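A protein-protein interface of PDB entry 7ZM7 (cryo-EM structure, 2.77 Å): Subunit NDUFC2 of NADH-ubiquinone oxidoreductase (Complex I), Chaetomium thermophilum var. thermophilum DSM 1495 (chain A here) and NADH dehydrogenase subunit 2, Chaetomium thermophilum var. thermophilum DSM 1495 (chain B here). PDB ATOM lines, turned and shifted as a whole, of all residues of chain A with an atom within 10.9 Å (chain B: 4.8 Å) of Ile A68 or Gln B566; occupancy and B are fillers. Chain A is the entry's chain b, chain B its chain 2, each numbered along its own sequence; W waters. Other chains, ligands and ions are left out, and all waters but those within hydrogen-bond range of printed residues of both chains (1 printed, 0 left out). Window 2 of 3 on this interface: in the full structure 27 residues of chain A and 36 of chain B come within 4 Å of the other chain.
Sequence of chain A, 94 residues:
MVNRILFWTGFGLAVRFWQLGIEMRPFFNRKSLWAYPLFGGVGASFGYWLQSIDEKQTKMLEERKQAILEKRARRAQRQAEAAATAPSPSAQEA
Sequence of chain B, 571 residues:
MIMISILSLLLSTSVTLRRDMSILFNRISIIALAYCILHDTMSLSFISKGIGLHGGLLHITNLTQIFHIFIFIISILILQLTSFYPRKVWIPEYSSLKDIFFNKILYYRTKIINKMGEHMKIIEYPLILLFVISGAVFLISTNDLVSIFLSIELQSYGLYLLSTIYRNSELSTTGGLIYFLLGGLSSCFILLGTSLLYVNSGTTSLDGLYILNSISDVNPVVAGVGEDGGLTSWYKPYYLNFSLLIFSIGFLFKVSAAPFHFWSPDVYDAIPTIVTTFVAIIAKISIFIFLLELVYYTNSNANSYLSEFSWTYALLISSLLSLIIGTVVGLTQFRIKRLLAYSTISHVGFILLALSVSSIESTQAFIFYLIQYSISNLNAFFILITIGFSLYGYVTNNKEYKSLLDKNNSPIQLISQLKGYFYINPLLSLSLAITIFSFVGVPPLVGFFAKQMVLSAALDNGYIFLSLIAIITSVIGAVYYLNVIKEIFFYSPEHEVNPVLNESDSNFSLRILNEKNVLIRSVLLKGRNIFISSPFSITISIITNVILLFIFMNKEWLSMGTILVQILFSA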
ATOM      1  N   GLN A  57       6.804 -11.901  26.019  1.00  0.00           N
ATOM      2  CA  GLN A  57       6.903 -10.726  25.164  1.00  0.00           C
ATOM      3  C   GLN A  57       7.325 -11.104  23.757  1.00  0.00           C
ATOM      4  O   GLN A  57       6.881 -10.495  22.779  1.00  0.00           O
ATOM      5  CB  GLN A  57       7.898  -9.742  25.763  1.00  0.00           C
ATOM      6  CG  GLN A  57       7.415  -9.073  27.021  1.00  0.00           C
ATOM      7  CD  GLN A  57       8.500  -8.317  27.725  1.00  0.00           C
ATOM      8  OE1 GLN A  57       8.238  -7.505  28.602  1.00  0.00           O
ATOM      9  NE2 GLN A  57       9.737  -8.591  27.353  1.00  0.00           N
ATOM     10  N   LYS A  59       6.642 -13.918  22.172  1.00  0.00           N
ATOM     11  CA  LYS A  59       5.487 -14.456  21.468  1.00  0.00           C
ATOM     12  C   LYS A  59       4.575 -13.340  20.989  1.00  0.00           C
ATOM     13  O   LYS A  59       4.052 -13.388  19.875  1.00  0.00           O
ATOM     14  CB  LYS A  59       4.734 -15.421  22.376  1.00  0.00           C
ATOM     15  CG  LYS A  59       5.206 -16.841  22.265  1.00  0.00           C
ATOM     16  CD  LYS A  59       4.191 -17.799  22.854  1.00  0.00           C
ATOM     17  CE  LYS A  59       4.078 -19.071  22.025  1.00  0.00           C
ATOM     18  NZ  LYS A  59       5.329 -19.876  22.058  1.00  0.00           N
ATOM     19  N   MET A  60       4.384 -12.322  21.823  1.00  0.00           N
ATOM     20  CA  MET A  60       3.485 -11.231  21.486  1.00  0.00           C
ATOM     21  C   MET A  60       4.036 -10.396  20.338  1.00  0.00           C
ATOM     22  O   MET A  60       3.325 -10.097  19.376  1.00  0.00           O
ATOM     23  CB  MET A  60       3.258 -10.377  22.720  1.00  0.00           C
ATOM     24  CG  MET A  60       2.188 -10.917  23.586  1.00  0.00           C
ATOM     25  SD  MET A  60       2.267 -10.340  25.279  1.00  0.00           S
ATOM     26  CE  MET A  60       0.707 -10.972  25.871  1.00  0.00           C
ATOM     27  N   LEU A  61       5.305 -10.015  20.416  1.00  0.00           N
ATOM     28  CA  LEU A  61       5.879  -9.239  19.331  1.00  0.00           C
ATOM     29  C   LEU A  61       5.917 -10.048  18.044  1.00  0.00           C
ATOM     30  O   LEU A  61       5.730  -9.496  16.956  1.00  0.00           O
ATOM     31  CB  LEU A  61       7.266  -8.744  19.721  1.00  0.00           C
ATOM     32  CG  LEU A  61       7.211  -7.753  20.884  1.00  0.00           C
ATOM     33  CD1 LEU A  61       8.588  -7.394  21.346  1.00  0.00           C
ATOM     34  CD2 LEU A  61       6.438  -6.516  20.509  1.00  0.00           C
ATOM     35  N   GLU A  62       6.130 -11.361  18.144  1.00  0.00           N
ATOM     36  CA  GLU A  62       6.057 -12.209  16.962  1.00  0.00           C
ATOM     37  C   GLU A  62       4.674 -12.160  16.331  1.00  0.00           C
ATOM     38  O   GLU A  62       4.539 -11.879  15.136  1.00  0.00           O
ATOM     39  CB  GLU A  62       6.429 -13.644  17.313  1.00  0.00           C
ATOM     40  CG  GLU A  62       7.916 -13.908  17.261  1.00  0.00           C
ATOM     41  CD  GLU A  62       8.508 -13.634  15.893  1.00  0.00           C
ATOM     42  OE1 GLU A  62       7.888 -14.031  14.884  1.00  0.00           O
ATOM     43  OE2 GLU A  62       9.589 -13.012  15.829  1.00  0.00           O
ATOM     44  N   GLU A  63       3.640 -12.451  17.115  1.00  0.00           N
ATOM     45  CA  GLU A  63       2.238 -12.372  16.626  1.00  0.00           C
ATOM     46  C   GLU A  63       1.974 -11.016  15.970  1.00  0.00           C
ATOM     47  O   GLU A  63       1.413 -11.015  14.874  1.00  0.00           O
ATOM     48  CB  GLU A  63       1.260 -12.605  17.776  1.00  0.00           C
ATOM     49  CG  GLU A  63       1.268 -14.025  18.307  1.00  0.00           C
ATOM     50  CD  GLU A  63       0.862 -15.095  17.307  1.00  0.00           C
ATOM     51  OE1 GLU A  63      -0.145 -14.894  16.596  1.00  0.00           O
ATOM     52  OE2 GLU A  63       1.559 -16.125  17.236  1.00  0.00           O
ATOM     53  N   ARG A  64       2.314  -9.907  16.634  1.00  0.00           N
ATOM     54  CA  ARG A  64       1.997  -8.557  16.109  1.00  0.00           C
ATOM     55  C   ARG A  64       2.689  -8.348  14.761  1.00  0.00           C
ATOM     56  O   ARG A  64       2.049  -7.816  13.860  1.00  0.00           O
ATOM     57  CB  ARG A  64       2.431  -7.489  17.113  1.00  0.00           C
ATOM     58  CG  ARG A  64       2.037  -6.071  16.736  1.00  0.00           C
ATOM     59  CD  ARG A  64       0.560  -5.824  16.947  1.00  0.00           C
ATOM     60  NE  ARG A  64       0.242  -4.454  16.593  1.00  0.00           N
ATOM     61  CZ  ARG A  64      -0.436  -4.094  15.516  1.00  0.00           C
ATOM     62  NH1 ARG A  64      -0.907  -5.010  14.690  1.00  0.00           N
ATOM     63  NH2 ARG A  64      -0.654  -2.817  15.283  1.00  0.00           N
ATOM     64  N   LYS A  65       3.945  -8.770  14.625  1.00  0.00           N
ATOM     65  CA  LYS A  65       4.648  -8.504  13.355  1.00  0.00           C
ATOM     66  C   LYS A  65       3.997  -9.338  12.261  1.00  0.00           C
ATOM     67  O   LYS A  65       4.090  -8.948  11.108  1.00  0.00           O
ATOM     68  CB  LYS A  65       6.138  -8.801  13.500  1.00  0.00           C
ATOM     69  CG  LYS A  65       6.891  -7.819  14.385  1.00  0.00           C
ATOM     70  CD  LYS A  65       8.321  -8.206  14.657  1.00  0.00           C
ATOM     71  CE  LYS A  65       8.469  -9.588  15.251  1.00  0.00           C
ATOM     72  NZ  LYS A  65       9.818  -9.796  15.823  1.00  0.00           N
ATOM     73  N   GLN A  66       3.345 -10.437  12.635  1.00  0.00           N
ATOM     74  CA  GLN A  66       2.604 -11.202  11.642  1.00  0.00           C
ATOM     75  C   GLN A  66       1.262 -10.557  11.333  1.00  0.00           C
ATOM     76  O   GLN A  66       0.808 -10.586  10.187  1.00  0.00           O
ATOM     77  CB  GLN A  66       2.429 -12.628  12.131  1.00  0.00           C
ATOM     78  CG  GLN A  66       3.737 -13.353  12.245  1.00  0.00           C
ATOM     79  CD  GLN A  66       4.428 -13.480  10.905  1.00  0.00           C
ATOM     80  OE1 GLN A  66       5.447 -12.838  10.656  1.00  0.00           O
ATOM     81  NE2 GLN A  66       3.868 -14.301  10.027  1.00  0.00           N
ATOM     82  N   ALA A  67       0.623  -9.954  12.336  1.00  0.00           N
ATOM     83  CA  ALA A  67      -0.625  -9.239  12.102  1.00  0.00           C
ATOM     84  C   ALA A  67      -0.422  -8.011  11.223  1.00  0.00           C
ATOM     85  O   ALA A  67      -1.227  -7.747  10.326  1.00  0.00           O
ATOM     86  CB  ALA A  67      -1.259  -8.841  13.427  1.00  0.00           C
ATOM     87  N   ILE A  68       0.629  -7.231  11.473  1.00  0.00           N
ATOM     88  CA  ILE A  68       0.894  -6.088  10.607  1.00  0.00           C
ATOM     89  C   ILE A  68       1.205  -6.573   9.201  1.00  0.00           C
ATOM     90  O   ILE A  68       1.028  -5.840   8.225  1.00  0.00           O
ATOM     91  CB  ILE A  68       2.028  -5.216  11.194  1.00  0.00           C
ATOM     92  CG1 ILE A  68       1.819  -4.969  12.682  1.00  0.00           C
ATOM     93  CG2 ILE A  68       2.087  -3.878  10.537  1.00  0.00           C
ATOM     94  CD1 ILE A  68       3.073  -4.532  13.405  1.00  0.00           C
ATOM     95  N   LEU A  69       1.661  -7.817   9.071  1.00  0.00           N
ATOM     96  CA  LEU A  69       1.951  -8.367   7.753  1.00  0.00           C
ATOM     97  C   LEU A  69       0.717  -8.983   7.105  1.00  0.00           C
ATOM     98  O   LEU A  69       0.765  -9.380   5.940  1.00  0.00           O
ATOM     99  CB  LEU A  69       3.073  -9.392   7.854  1.00  0.00           C
ATOM    100  CG  LEU A  69       4.420  -8.725   8.049  1.00  0.00           C
ATOM    101  CD1 LEU A  69       5.520  -9.735   8.133  1.00  0.00           C
ATOM    102  CD2 LEU A  69       4.671  -7.752   6.946  1.00  0.00           C
ATOM    103  N   GLU A  70      -0.379  -9.117   7.848  1.00  0.00           N
ATOM    104  CA  GLU A  70      -1.656  -9.416   7.206  1.00  0.00           C
ATOM    105  C   GLU A  70      -2.363  -8.141   6.787  1.00  0.00           C
ATOM    106  O   GLU A  70      -2.868  -8.040   5.668  1.00  0.00           O
ATOM    107  CB  GLU A  70      -2.555 -10.239   8.126  1.00  0.00           C
ATOM    108  CG  GLU A  70      -1.854 -11.300   8.942  1.00  0.00           C
ATOM    109  CD  GLU A  70      -1.189 -12.386   8.104  1.00  0.00           C
ATOM    110  OE1 GLU A  70      -1.342 -12.394   6.866  1.00  0.00           O
ATOM    111  OE2 GLU A  70      -0.502 -13.247   8.691  1.00  0.00           O
ATOM    112  N   LYS A  71      -2.389  -7.151   7.667  1.00  0.00           N
ATOM    113  CA  LYS A  71      -3.080  -5.913   7.352  1.00  0.00           C
ATOM    114  C   LYS A  71      -2.500  -5.270   6.102  1.00  0.00           C
ATOM    115  O   LYS A  71      -3.242  -4.845   5.211  1.00  0.00           O
ATOM    116  CB  LYS A  71      -3.000  -4.967   8.546  1.00  0.00           C
ATOM    117  CG  LYS A  71      -3.868  -3.750   8.412  1.00  0.00           C
ATOM    118  CD  LYS A  71      -4.162  -3.132   9.756  1.00  0.00           C
ATOM    119  CE  LYS A  71      -4.877  -1.812   9.580  1.00  0.00           C
ATOM    120  NZ  LYS A  71      -6.046  -1.966   8.675  1.00  0.00           N
ATOM    121  N   ARG A  72      -1.173  -5.207   6.013  1.00  0.00           N
ATOM    122  CA  ARG A  72      -0.536  -4.705   4.807  1.00  0.00           C
ATOM    123  C   ARG A  72      -0.802  -5.616   3.622  1.00  0.00           C
ATOM    124  O   ARG A  72      -0.966  -5.137   2.495  1.00  0.00           O
ATOM    125  CB  ARG A  72       0.961  -4.566   5.028  1.00  0.00           C
ATOM    126  CG  ARG A  72       1.355  -3.566   6.082  1.00  0.00           C
ATOM    127  CD  ARG A  72       2.801  -3.218   5.921  1.00  0.00           C
ATOM    128  NE  ARG A  72       3.072  -2.730   4.577  1.00  0.00           N
ATOM    129  CZ  ARG A  72       2.831  -1.488   4.169  1.00  0.00           C
ATOM    130  NH1 ARG A  72       2.313  -0.597   4.999  1.00  0.00           N
ATOM    131  NH2 ARG A  72       3.116  -1.133   2.929  1.00  0.00           N
ATOM    132  N   ALA A  73      -0.850  -6.927   3.849  1.00  0.00           N
ATOM    133  CA  ALA A  73      -1.117  -7.852   2.759  1.00  0.00           C
ATOM    134  C   ALA A  73      -2.565  -7.774   2.302  1.00  0.00           C
ATOM    135  O   ALA A  73      -2.836  -7.556   1.120  1.00  0.00           O
ATOM    136  CB  ALA A  73      -0.772  -9.277   3.190  1.00  0.00           C
ATOM    137  N   ARG A  74      -3.507  -7.934   3.228  1.00  0.00           N
ATOM    138  CA  ARG A  74      -4.914  -8.006   2.855  1.00  0.00           C
ATOM    139  C   ARG A  74      -5.387  -6.718   2.214  1.00  0.00           C
ATOM    140  O   ARG A  74      -6.261  -6.739   1.344  1.00  0.00           O
ATOM    141  CB  ARG A  74      -5.764  -8.328   4.078  1.00  0.00           C
ATOM    142  CG  ARG A  74      -5.783  -9.790   4.460  1.00  0.00           C
ATOM    143  CD  ARG A  74      -6.688  -9.991   5.649  1.00  0.00           C
ATOM    144  NE  ARG A  74      -6.195  -9.247   6.799  1.00  0.00           N
ATOM    145  CZ  ARG A  74      -6.795  -8.182   7.317  1.00  0.00           C
ATOM    146  NH1 ARG A  74      -7.922  -7.732   6.783  1.00  0.00           N
ATOM    147  NH2 ARG A  74      -6.269  -7.567   8.367  1.00  0.00           N
ATOM    148  N   ARG A  75      -4.853  -5.579   2.653  1.00  0.00           N
ATOM    149  CA  ARG A  75      -5.190  -4.319   2.008  1.00  0.00           C
ATOM    150  C   ARG A  75      -4.704  -4.301   0.573  1.00  0.00           C
ATOM    151  O   ARG A  75      -5.424  -3.863  -0.329  1.00  0.00           O
ATOM    152  CB  ARG A  75      -4.598  -3.149   2.790  1.00  0.00           C
ATOM    153  CG  ARG A  75      -4.961  -1.787   2.225  1.00  0.00           C
ATOM    154  CD  ARG A  75      -4.020  -0.701   2.717  1.00  0.00           C
ATOM    155  NE  ARG A  75      -4.022  -0.581   4.173  1.00  0.00           N
ATOM    156  CZ  ARG A  75      -5.004  -0.031   4.880  1.00  0.00           C
ATOM    157  NH1 ARG A  75      -6.073   0.459   4.270  1.00  0.00           N
ATOM    158  NH2 ARG A  75      -4.915   0.033   6.202  1.00  0.00           N
ATOM    159  N   ALA A  76      -3.483  -4.776   0.336  1.00  0.00           N
ATOM    160  CA  ALA A  76      -2.974  -4.837  -1.024  1.00  0.00           C
ATOM    161  C   ALA A  76      -3.794  -5.792  -1.871  1.00  0.00           C
ATOM    162  O   ALA A  76      -3.958  -5.573  -3.076  1.00  0.00           O
ATOM    163  CB  ALA A  76      -1.505  -5.253  -1.021  1.00  0.00           C
ATOM    164  N   ILE B 360       3.918   6.144  17.066  1.00  0.00           N
ATOM    165  CA  ILE B 360       4.246   4.895  17.798  1.00  0.00           C
ATOM    166  C   ILE B 360       5.582   5.095  18.538  1.00  0.00           C
ATOM    167  O   ILE B 360       5.629   4.794  19.738  1.00  0.00           O
ATOM    168  CB  ILE B 360       4.275   3.699  16.810  1.00  0.00           C
ATOM    169  CG1 ILE B 360       2.992   3.616  15.983  1.00  0.00           C
ATOM    170  CG2 ILE B 360       4.566   2.392  17.527  1.00  0.00           C
ATOM    171  CD1 ILE B 360       2.821   2.314  15.250  1.00  0.00           C
ATOM    172  N   GLN B 364       6.162   5.235  22.893  1.00  0.00           N
ATOM    173  CA  GLN B 364       7.120   4.299  23.536  1.00  0.00           C
ATOM    174  C   GLN B 364       8.181   5.115  24.271  1.00  0.00           C
ATOM    175  O   GLN B 364       8.566   4.716  25.377  1.00  0.00           O
ATOM    176  CB  GLN B 364       7.750   3.385  22.489  1.00  0.00           C
ATOM    177  CG  GLN B 364       6.809   2.363  21.885  1.00  0.00           C
ATOM    178  CD  GLN B 364       7.378   1.836  20.593  1.00  0.00           C
ATOM    179  OE1 GLN B 364       6.728   1.095  19.863  1.00  0.00           O
ATOM    180  NE2 GLN B 364       8.603   2.236  20.301  1.00  0.00           N
ATOM    181  N   THR B 562       6.997  -1.248  24.029  1.00  0.00           N
ATOM    182  CA  THR B 562       6.720  -1.525  22.596  1.00  0.00           C
ATOM    183  C   THR B 562       5.400  -2.289  22.465  1.00  0.00           C
ATOM    184  O   THR B 562       4.629  -1.929  21.572  1.00  0.00           O
ATOM    185  CB  THR B 562       7.930  -2.108  21.851  1.00  0.00           C
ATOM    186  OG1 THR B 562       7.749  -1.835  20.461  1.00  0.00           O
ATOM    187  CG2 THR B 562       8.127  -3.595  22.042  1.00  0.00           C
ATOM    188  N   ILE B 563       5.137  -3.255  23.350  1.00  0.00           N
ATOM    189  CA  ILE B 563       3.849  -4.008  23.334  1.00  0.00           C
ATOM    190  C   ILE B 563       2.718  -3.063  23.745  1.00  0.00           C
ATOM    191  O   ILE B 563       1.650  -3.118  23.111  1.00  0.00           O
ATOM    192  CB  ILE B 563       3.912  -5.245  24.244  1.00  0.00           C
ATOM    193  CG1 ILE B 563       5.071  -6.169  23.870  1.00  0.00           C
ATOM    194  CG2 ILE B 563       2.587  -5.992  24.244  1.00  0.00           C
ATOM    195  CD1 ILE B 563       5.112  -7.442  24.670  1.00  0.00           C
ATOM    196  N   LEU B 564       2.940  -2.221  24.752  1.00  0.00           N
ATOM    197  CA  LEU B 564       1.843  -1.372  25.198  1.00  0.00           C
ATOM    198  C   LEU B 564       1.409  -0.415  24.106  1.00  0.00           C
ATOM    199  O   LEU B 564       0.211  -0.224  23.880  1.00  0.00           O
ATOM    200  CB  LEU B 564       2.233  -0.597  26.451  1.00  0.00           C
ATOM    201  CG  LEU B 564       2.262  -1.377  27.752  1.00  0.00           C
ATOM    202  CD1 LEU B 564       2.694  -0.488  28.873  1.00  0.00           C
ATOM    203  CD2 LEU B 564       0.919  -1.950  28.018  1.00  0.00           C
ATOM    204  N   VAL B 565       2.353   0.123  23.347  1.00  0.00           N
ATOM    205  CA  VAL B 565       1.934   1.122  22.330  1.00  0.00           C
ATOM    206  C   VAL B 565       1.423   0.353  21.103  1.00  0.00           C
ATOM    207  O   VAL B 565       0.645   0.924  20.338  1.00  0.00           O
ATOM    208  CB  VAL B 565       3.110   2.076  22.050  1.00  0.00           C
ATOM    209  CG1 VAL B 565       2.834   3.051  20.920  1.00  0.00           C
ATOM    210  CG2 VAL B 565       3.512   2.820  23.310  1.00  0.00           C
ATOM    211  N   GLN B 566       1.798  -0.920  20.962  1.00  0.00           N
ATOM    212  CA  GLN B 566       1.327  -1.762  19.834  1.00  0.00           C
ATOM    213  C   GLN B 566      -0.177  -1.973  19.959  1.00  0.00           C
ATOM    214  O   GLN B 566      -0.808  -2.095  18.928  1.00  0.00           O
ATOM    215  CB  GLN B 566       2.140  -3.048  19.646  1.00  0.00           C
ATOM    216  CG  GLN B 566       3.432  -2.870  18.858  1.00  0.00           C
ATOM    217  CD  GLN B 566       3.293  -2.073  17.585  1.00  0.00           C
ATOM    218  OE1 GLN B 566       2.487  -2.379  16.712  1.00  0.00           O
ATOM    219  NE2 GLN B 566       4.113  -1.045  17.458  1.00  0.00           N
ATOM    220  N   ILE B 567      -0.705  -1.996  21.176  1.00  0.00           N
ATOM    221  CA  ILE B 567      -2.156  -2.221  21.418  1.00  0.00           C
ATOM    222  C   ILE B 567      -2.882  -0.884  21.262  1.00  0.00           C
ATOM    223  O   ILE B 567      -3.873  -0.837  20.535  1.00  0.00           O
ATOM    224  CB  ILE B 567      -2.401  -2.858  22.800  1.00  0.00           C
ATOM    225  CG1 ILE B 567      -1.687  -4.205  22.934  1.00  0.00           C
ATOM    226  CG2 ILE B 567      -3.884  -2.973  23.100  1.00  0.00           C
ATOM    227  CD1 ILE B 567      -1.546  -4.693  24.354  1.00  0.00           C
ATOM    228  N   LEU B 568      -2.417   0.173  21.917  1.00  0.00           N
ATOM    229  CA  LEU B 568      -3.071   1.503  21.823  1.00  0.00           C
ATOM    230  C   LEU B 568      -3.217   1.916  20.362  1.00  0.00           C
ATOM    231  O   LEU B 568      -4.176   2.612  20.076  1.00  0.00           O
ATOM    232  CB  LEU B 568      -2.249   2.538  22.599  1.00  0.00           C
ATOM    233  CG  LEU B 568      -2.641   3.994  22.356  1.00  0.00           C
ATOM    234  CD1 LEU B 568      -4.081   4.245  22.768  1.00  0.00           C
ATOM    235  CD2 LEU B 568      -1.702   4.943  23.079  1.00  0.00           C
ATOM    236  N   PHE B 569      -2.262   1.570  19.500  1.00  0.00           N
ATOM    237  CA  PHE B 569      -2.278   1.960  18.063  1.00  0.00           C
ATOM    238  C   PHE B 569      -2.826   0.830  17.197  1.00  0.00           C
ATOM    239  O   PHE B 569      -3.138   1.114  16.043  1.00  0.00           O
ATOM    240  CB  PHE B 569      -0.860   2.307  17.611  1.00  0.00           C
ATOM    241  CG  PHE B 569      -0.434   3.730  17.867  1.00  0.00           C
ATOM    242  CD1 PHE B 569      -0.115   4.158  19.145  1.00  0.00           C
ATOM    243  CD2 PHE B 569      -0.337   4.639  16.827  1.00  0.00           C
ATOM    244  CE1 PHE B 569       0.274   5.466  19.381  1.00  0.00           C
ATOM    245  CE2 PHE B 569       0.055   5.947  17.063  1.00  0.00           C
ATOM    246  CZ  PHE B 569       0.357   6.358  18.338  1.00  0.00           C
ATOM    247  N   SER B 570      -3.062  -0.354  17.763  1.00  0.00           N
ATOM    248  CA  SER B 570      -3.461  -1.567  16.998  1.00  0.00           C
ATOM    249  C   SER B 570      -4.764  -1.364  16.247  1.00  0.00           C
ATOM    250  O   SER B 570      -5.588  -0.567  16.709  1.00  0.00           O
ATOM    251  CB  SER B 570      -3.620  -2.730  17.899  1.00  0.00           C
ATOM    252  OG  SER B 570      -4.746  -2.555  18.743  1.00  0.00           O
HETATM  253  O   HOH W   1      -1.760  -0.557  13.974  1.00  0.00           O
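The side-chain amide oxygen of Gln B364 sits at hydrogen-bond distance from the side-chain hydroxyl of Thr B562 (3.2 Å).
The backbone carbonyl oxygen (O) of Ile B567 sits at hydrogen-bond distance from the side-chain hydroxyl (OG) of Ser B570, at 2.6 Å.
Water W1 bridges the guanidinium group of Arg A64 (2.8 Å) and the backbone carbonyl oxygen of Phe B569 (3.0 Å).
Of the printed residues of chain B, Gln A57 touches Ile B563 (3.7 Å).
Printed residues of chain B within 4 Å of Met A60: Ile B563.
Printed residues of chain B within 4 Å of Leu A61: Thr B562 (3.7 Å) and Ile B563 (3.6 Å).
Glu A62 touches none of the printed residues of chain B.
Printed residues of chain B within 4 Å of Ile A68: Gln B566 (3.99 Å).
Ile B360 touches none of the printed residues of chain A.
Of chain A, only Leu A61 comes within 4 Å of Thr B562.
Printed residues of chain A within 4 Å of Ile B563: Gln A57, Met A60 and Leu A61.
No residue of chain A comes within 4 Å of Val B565.
Printed residues of chain A within 4 Å of Gln B566: Arg A64 (3.1 Å) and Ile A68 (3.99 Å).
No residue of chain A comes within 4 Å of Ile B567.
Ser B570 touches just one residue of chain A: Arg A64.
The nearest printed residue of chain B that does not touch Ile A68 is Ile B360 (7.1 Å).
The nearest printed residue of chain B that does not touch Leu A61 is Gln B566 (5.0 Å).
The side-chain amide oxygen (OE1) of Gln B566 sits at hydrogen-bond distance from the guanidinium group (NE) of Arg A64.
Among the printed residues, merely in contact across the chains: Gln A57 with Ile B563 (3.7 Å), Met A60 with Ile B563 (3.98 Å), Leu A61 with Thr B562 (3.7 Å), Leu A61 with Ile B563 (3.6 Å), Arg A64 with Ser B570 (3.5 Å) and Ile A68 with Gln B566 (3.99 Å).
Printed residues of chain B that touch a printed residue of chain A: Thr B562, Ile B563, Gln B566 and Ser B570.
Hydrophobic or aromatic side chains of chain B within 4 Å of the printed part of chain A: Ile B563.
Of the 19 printed residues of chain A, 5 touch a printed residue of chain B.
Hydrophobic or aromatic side chains of chain A that line the printed part of chain B: Met A60, Leu A61 and Ile A68.
Among the printed residues, 7 pairs touch across the chains.
Among the printed residues, no Asp or Glu carboxylate lies within 4 Å of a Lys or Arg side-chain nitrogen of the other chain.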
